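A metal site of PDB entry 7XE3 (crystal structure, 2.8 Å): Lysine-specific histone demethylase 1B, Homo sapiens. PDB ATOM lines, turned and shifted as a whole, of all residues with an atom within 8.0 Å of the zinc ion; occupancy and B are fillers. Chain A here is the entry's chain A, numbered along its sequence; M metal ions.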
ATOM      1  N   GLN A 112      -7.940  -2.671  34.212  1.00  0.00           N
ATOM      2  CA  GLN A 112      -8.447  -1.340  33.920  1.00  0.00           C
ATOM      3  C   GLN A 112      -8.518  -1.074  32.435  1.00  0.00           C
ATOM      4  O   GLN A 112      -7.651  -1.510  31.670  1.00  0.00           O
ATOM      5  CB  GLN A 112      -7.585  -0.248  34.537  1.00  0.00           C
ATOM      6  CG  GLN A 112      -7.432  -0.365  36.004  1.00  0.00           C
ATOM      7  CD  GLN A 112      -6.266   0.442  36.493  1.00  0.00           C
ATOM      8  OE1 GLN A 112      -5.094   0.079  36.267  1.00  0.00           O
ATOM      9  NE2 GLN A 112      -6.567   1.563  37.161  1.00  0.00           N
ATOM     10  N   CYS A 113      -9.535  -0.344  32.020  1.00  0.00           N
ATOM     11  CA  CYS A 113      -9.522   0.203  30.688  1.00  0.00           C
ATOM     12  C   CYS A 113      -8.287   1.087  30.540  1.00  0.00           C
ATOM     13  O   CYS A 113      -7.986   1.899  31.420  1.00  0.00           O
ATOM     14  CB  CYS A 113     -10.802   0.985  30.444  1.00  0.00           C
ATOM     15  SG  CYS A 113     -11.064   1.427  28.746  1.00  0.00           S
ATOM     16  N   THR A 114      -7.529   0.887  29.450  1.00  0.00           N
ATOM     17  CA  THR A 114      -6.326   1.674  29.212  1.00  0.00           C
ATOM     18  C   THR A 114      -6.598   3.008  28.530  1.00  0.00           C
ATOM     19  O   THR A 114      -5.715   3.867  28.519  1.00  0.00           O
ATOM     20  CB  THR A 114      -5.300   0.887  28.381  1.00  0.00           C
ATOM     21  OG1 THR A 114      -5.843   0.560  27.092  1.00  0.00           O
ATOM     22  CG2 THR A 114      -4.900  -0.390  29.101  1.00  0.00           C
ATOM     23  N   LYS A 115      -7.795   3.196  27.960  1.00  0.00           N
ATOM     24  CA  LYS A 115      -8.204   4.503  27.486  1.00  0.00           C
ATOM     25  C   LYS A 115      -7.994   5.532  28.589  1.00  0.00           C
ATOM     26  O   LYS A 115      -8.354   5.279  29.742  1.00  0.00           O
ATOM     27  CB  LYS A 115      -9.676   4.461  27.067  1.00  0.00           C
ATOM     28  CG  LYS A 115     -10.142   5.540  26.108  1.00  0.00           C
ATOM     29  CD  LYS A 115     -11.646   5.717  26.233  1.00  0.00           C
ATOM     30  CE  LYS A 115     -12.346   5.928  24.901  1.00  0.00           C
ATOM     31  NZ  LYS A 115     -13.822   6.013  25.088  1.00  0.00           N
ATOM     32  N   PRO A 116      -7.379   6.682  28.301  1.00  0.00           N
ATOM     33  CA  PRO A 116      -6.995   7.601  29.393  1.00  0.00           C
ATOM     34  C   PRO A 116      -8.167   8.185  30.169  1.00  0.00           C
ATOM     35  O   PRO A 116      -8.140   8.191  31.415  1.00  0.00           O
ATOM     36  CB  PRO A 116      -6.194   8.698  28.663  1.00  0.00           C
ATOM     37  CG  PRO A 116      -6.628   8.611  27.225  1.00  0.00           C
ATOM     38  CD  PRO A 116      -6.891   7.151  26.995  1.00  0.00           C
ATOM     39  N   GLU A 117      -9.206   8.694  29.495  1.00  0.00           N
ATOM     40  CA  GLU A 117     -10.313   9.349  30.169  1.00  0.00           C
ATOM     41  C   GLU A 117     -11.321   8.367  30.772  1.00  0.00           C
ATOM     42  O   GLU A 117     -12.349   8.815  31.300  1.00  0.00           O
ATOM     43  CB  GLU A 117     -11.038  10.312  29.212  1.00  0.00           C
ATOM     44  CG  GLU A 117     -11.776   9.617  28.067  1.00  0.00           C
ATOM     45  CD  GLU A 117     -10.885   9.350  26.870  1.00  0.00           C
ATOM     46  OE1 GLU A 117      -9.662   9.591  26.961  1.00  0.00           O
ATOM     47  OE2 GLU A 117     -11.420   8.903  25.826  1.00  0.00           O
ATOM     48  N   CYS A 118     -11.039   7.066  30.724  1.00  0.00           N
ATOM     49  CA  CYS A 118     -11.929   6.038  31.278  1.00  0.00           C
ATOM     50  C   CYS A 118     -11.303   5.392  32.513  1.00  0.00           C
ATOM     51  O   CYS A 118     -11.727   5.666  33.632  1.00  0.00           O
ATOM     52  CB  CYS A 118     -12.256   4.993  30.213  1.00  0.00           C
ATOM     53  SG  CYS A 118     -13.341   3.677  30.793  1.00  0.00           S
ATOM     54  N   ARG A 119     -10.324   4.507  32.327  1.00  0.00           N
ATOM     55  CA  ARG A 119      -9.565   3.888  33.423  1.00  0.00           C
ATOM     56  C   ARG A 119     -10.450   3.043  34.347  1.00  0.00           C
ATOM     57  O   ARG A 119     -10.048   2.735  35.470  1.00  0.00           O
ATOM     58  CB  ARG A 119      -8.784   4.940  34.230  1.00  0.00           C
ATOM     59  CG  ARG A 119      -7.685   5.664  33.465  1.00  0.00           C
ATOM     60  CD  ARG A 119      -6.548   4.705  33.106  1.00  0.00           C
ATOM     61  NE  ARG A 119      -5.641   4.495  34.226  1.00  0.00           N
ATOM     62  CZ  ARG A 119      -4.838   3.436  34.362  1.00  0.00           C
ATOM     63  NH1 ARG A 119      -4.856   2.441  33.480  1.00  0.00           N
ATOM     64  NH2 ARG A 119      -4.017   3.382  35.409  1.00  0.00           N
ATOM     65  N   LYS A 120     -11.646   2.652  33.875  1.00  0.00           N
ATOM     66  CA  LYS A 120     -12.592   1.897  34.686  1.00  0.00           C
ATOM     67  C   LYS A 120     -12.161   0.431  34.844  1.00  0.00           C
ATOM     68  O   LYS A 120     -11.614  -0.184  33.934  1.00  0.00           O
ATOM     69  CB  LYS A 120     -14.001   1.950  34.064  1.00  0.00           C
ATOM     70  CG  LYS A 120     -14.749   3.237  34.322  1.00  0.00           C
ATOM     71  CD  LYS A 120     -16.076   3.290  33.570  1.00  0.00           C
ATOM     72  CE  LYS A 120     -16.788   4.610  33.838  1.00  0.00           C
ATOM     73  NZ  LYS A 120     -17.947   4.872  32.932  1.00  0.00           N
ATOM     74  N   TRP A 121     -12.450  -0.119  36.022  1.00  0.00           N
ATOM     75  CA  TRP A 121     -12.136  -1.510  36.310  1.00  0.00           C
ATOM     76  C   TRP A 121     -13.197  -2.439  35.748  1.00  0.00           C
ATOM     77  O   TRP A 121     -14.401  -2.173  35.838  1.00  0.00           O
ATOM     78  CB  TRP A 121     -12.032  -1.716  37.820  1.00  0.00           C
ATOM     79  CG  TRP A 121     -10.750  -1.237  38.401  1.00  0.00           C
ATOM     80  CD1 TRP A 121     -10.536  -0.078  39.090  1.00  0.00           C
ATOM     81  CD2 TRP A 121      -9.481  -1.909  38.350  1.00  0.00           C
ATOM     82  NE1 TRP A 121      -9.225   0.006  39.471  1.00  0.00           N
ATOM     83  CE2 TRP A 121      -8.555  -1.101  39.036  1.00  0.00           C
ATOM     84  CE3 TRP A 121      -9.045  -3.112  37.796  1.00  0.00           C
ATOM     85  CZ2 TRP A 121      -7.233  -1.465  39.169  1.00  0.00           C
ATOM     86  CZ3 TRP A 121      -7.741  -3.466  37.938  1.00  0.00           C
ATOM     87  CH2 TRP A 121      -6.836  -2.651  38.620  1.00  0.00           C
ATOM     88  N   ARG A 122     -12.751  -3.549  35.160  1.00  0.00           N
ATOM     89  CA  ARG A 122     -13.640  -4.570  34.619  1.00  0.00           C
ATOM     90  C   ARG A 122     -13.173  -5.955  35.063  1.00  0.00           C
ATOM     91  O   ARG A 122     -11.984  -6.167  35.314  1.00  0.00           O
ATOM     92  CB  ARG A 122     -13.713  -4.543  33.090  1.00  0.00           C
ATOM     93  CG  ARG A 122     -14.144  -3.235  32.484  1.00  0.00           C
ATOM     94  CD  ARG A 122     -15.419  -2.719  33.073  1.00  0.00           C
ATOM     95  NE  ARG A 122     -15.894  -1.574  32.310  1.00  0.00           N
ATOM     96  CZ  ARG A 122     -16.877  -0.791  32.684  1.00  0.00           C
ATOM     97  NH1 ARG A 122     -17.460  -0.942  33.865  1.00  0.00           N
ATOM     98  NH2 ARG A 122     -17.301   0.169  31.860  1.00  0.00           N
ATOM     99  N   TYR A 138      -5.847  -3.251  27.290  1.00  0.00           N
ATOM    100  CA  TYR A 138      -7.259  -3.552  27.502  1.00  0.00           C
ATOM    101  C   TYR A 138      -8.132  -2.303  27.353  1.00  0.00           C
ATOM    102  O   TYR A 138      -7.802  -1.232  27.870  1.00  0.00           O
ATOM    103  CB  TYR A 138      -7.501  -4.146  28.889  1.00  0.00           C
ATOM    104  CG  TYR A 138      -8.955  -4.466  29.111  1.00  0.00           C
ATOM    105  CD1 TYR A 138      -9.540  -5.556  28.486  1.00  0.00           C
ATOM    106  CD2 TYR A 138      -9.759  -3.668  29.916  1.00  0.00           C
ATOM    107  CE1 TYR A 138     -10.878  -5.856  28.662  1.00  0.00           C
ATOM    108  CE2 TYR A 138     -11.115  -3.957  30.101  1.00  0.00           C
ATOM    109  CZ  TYR A 138     -11.663  -5.059  29.462  1.00  0.00           C
ATOM    110  OH  TYR A 138     -12.990  -5.383  29.611  1.00  0.00           O
ATOM    111  N   ARG A 139      -9.255  -2.474  26.672  1.00  0.00           N
ATOM    112  CA  ARG A 139     -10.291  -1.452  26.574  1.00  0.00           C
ATOM    113  C   ARG A 139     -11.655  -2.100  26.780  1.00  0.00           C
ATOM    114  O   ARG A 139     -11.923  -3.185  26.265  1.00  0.00           O
ATOM    115  CB  ARG A 139     -10.229  -0.743  25.214  1.00  0.00           C
ATOM    116  CG  ARG A 139      -9.119   0.279  25.140  1.00  0.00           C
ATOM    117  CD  ARG A 139      -9.027   0.886  23.767  1.00  0.00           C
ATOM    118  NE  ARG A 139      -8.506   2.240  23.822  1.00  0.00           N
ATOM    119  CZ  ARG A 139      -8.282   3.009  22.759  1.00  0.00           C
ATOM    120  NH1 ARG A 139      -8.500   2.572  21.531  1.00  0.00           N
ATOM    121  NH2 ARG A 139      -7.843   4.251  22.943  1.00  0.00           N
ATOM    122  N   CYS A 140     -12.512  -1.400  27.532  1.00  0.00           N
ATOM    123  CA  CYS A 140     -13.821  -1.884  27.983  1.00  0.00           C
ATOM    124  C   CYS A 140     -14.559  -2.686  26.920  1.00  0.00           C
ATOM    125  O   CYS A 140     -14.768  -2.220  25.807  1.00  0.00           O
ATOM    126  CB  CYS A 140     -14.671  -0.690  28.408  1.00  0.00           C
ATOM    127  SG  CYS A 140     -14.153   0.042  29.948  1.00  0.00           S
ATOM    128  N   GLY A 141     -14.960  -3.903  27.302  1.00  0.00           N
ATOM    129  CA  GLY A 141     -15.873  -4.687  26.489  1.00  0.00           C
ATOM    130  C   GLY A 141     -15.358  -5.110  25.124  1.00  0.00           C
ATOM    131  O   GLY A 141     -16.164  -5.441  24.240  1.00  0.00           O
ATOM    132  N   SER A 153     -16.796   3.112  21.055  1.00  0.00           N
ATOM    133  CA  SER A 153     -16.389   3.497  22.401  1.00  0.00           C
ATOM    134  C   SER A 153     -17.580   3.515  23.355  1.00  0.00           C
ATOM    135  O   SER A 153     -17.603   4.303  24.310  1.00  0.00           O
ATOM    136  CB  SER A 153     -15.704   4.868  22.398  1.00  0.00           C
ATOM    137  OG  SER A 153     -14.374   4.788  21.911  1.00  0.00           O
ATOM    138  N   ASP A 154     -18.557   2.653  23.109  1.00  0.00           N
ATOM    139  CA  ASP A 154     -19.796   2.659  23.872  1.00  0.00           C
ATOM    140  C   ASP A 154     -19.645   2.004  25.241  1.00  0.00           C
ATOM    141  O   ASP A 154     -20.288   2.430  26.209  1.00  0.00           O
ATOM    142  CB  ASP A 154     -20.893   1.965  23.073  1.00  0.00           C
ATOM    143  CG  ASP A 154     -22.188   2.737  23.067  1.00  0.00           C
ATOM    144  OD1 ASP A 154     -22.440   3.474  24.040  1.00  0.00           O
ATOM    145  OD2 ASP A 154     -22.957   2.599  22.093  1.00  0.00           O
ATOM    146  N   HIS A 155     -18.817   0.956  25.343  1.00  0.00           N
ATOM    147  CA  HIS A 155     -18.722   0.133  26.544  1.00  0.00           C
ATOM    148  C   HIS A 155     -18.058   0.839  27.721  1.00  0.00           C
ATOM    149  O   HIS A 155     -18.100   0.319  28.844  1.00  0.00           O
ATOM    150  CB  HIS A 155     -17.931  -1.145  26.248  1.00  0.00           C
ATOM    151  CG  HIS A 155     -18.699  -2.174  25.484  1.00  0.00           C
ATOM    152  ND1 HIS A 155     -19.197  -3.314  26.075  1.00  0.00           N
ATOM    153  CD2 HIS A 155     -19.029  -2.252  24.168  1.00  0.00           C
ATOM    154  CE1 HIS A 155     -19.809  -4.044  25.161  1.00  0.00           C
ATOM    155  NE2 HIS A 155     -19.726  -3.426  24.002  1.00  0.00           N
ATOM    156  N   CYS A 156     -17.412   1.982  27.481  1.00  0.00           N
ATOM    157  CA  CYS A 156     -16.721   2.658  28.568  1.00  0.00           C
ATOM    158  C   CYS A 156     -17.695   3.298  29.541  1.00  0.00           C
ATOM    159  O   CYS A 156     -17.473   3.267  30.752  1.00  0.00           O
ATOM    160  CB  CYS A 156     -15.762   3.702  27.996  1.00  0.00           C
ATOM    161  SG  CYS A 156     -14.317   2.962  27.211  1.00  0.00           S
ATOM    162  N   SER A 157     -18.781   3.876  29.026  1.00  0.00           N
ATOM    163  CA  SER A 157     -19.733   4.598  29.843  1.00  0.00           C
ATOM    164  C   SER A 157     -20.485   3.696  30.826  1.00  0.00           C
ATOM    165  O   SER A 157     -21.172   4.234  31.700  1.00  0.00           O
ATOM    166  CB  SER A 157     -20.745   5.309  28.948  1.00  0.00           C
ATOM    167  OG  SER A 157     -20.146   6.407  28.281  1.00  0.00           O
ATOM    168  N   LEU A 158     -20.377   2.374  30.710  1.00  0.00           N
ATOM    169  CA  LEU A 158     -21.089   1.504  31.632  1.00  0.00           C
ATOM    170  C   LEU A 158     -20.497   1.622  33.032  1.00  0.00           C
ATOM    171  O   LEU A 158     -19.278   1.779  33.182  1.00  0.00           O
ATOM    172  CB  LEU A 158     -21.050   0.042  31.205  1.00  0.00           C
ATOM    173  CG  LEU A 158     -21.898  -0.356  30.007  1.00  0.00           C
ATOM    174  CD1 LEU A 158     -22.114  -1.854  30.069  1.00  0.00           C
ATOM    175  CD2 LEU A 158     -23.216   0.400  29.997  1.00  0.00           C
HETATM  176 ZN    ZN M   1     -13.301   2.041  29.129  1.00  0.00          ZN
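The side-chain sulfur (SG) of Cys 140 sits close to the guanidinium group (NE) of Arg 122, 3.3 Å away.
The side-chain sulfur (SG) of Cys 118 sits close to the backbone NH (N) of Lys 120, 3.7 Å away.
The side-chain sulfur (SG) of Cys 113 sits close to the backbone NH (N) of Lys 115, at 3.8 Å.
N of Cys 113 lies within hydrogen-bond range of O of Lys 120, 2.8 Å away.
The side-chain sulfur (SG) of Cys 156 sits close to the side-chain amino group (NZ) of Lys 115.
The side-chain amino group (NZ) of Lys 120 sits at hydrogen-bond distance from the backbone carbonyl oxygen (O) of Cys 156 (2.7 Å).
O of Cys 156 sits at hydrogen-bond distance from NH2 of Arg 122 (3.3 Å).
The side-chain sulfur (SG) of Cys 140 is bound to the zinc ion (2.3 Å).
SG of Cys 118 is bound to the zinc ion (2.3 Å).
The side-chain sulfur (SG) of Cys 113 binds the zinc ion (2.4 Å).
The side-chain sulfur (SG) of Cys 156 binds the zinc ion, 2.4 Å away.
The zinc ion has four donor atoms within binding distance.
Of the 21 residues printed, 4 come within 4 Å of the zinc ion.
The nearest printed residue that does not touch the zinc ion is Lys 115 (4.8 Å).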
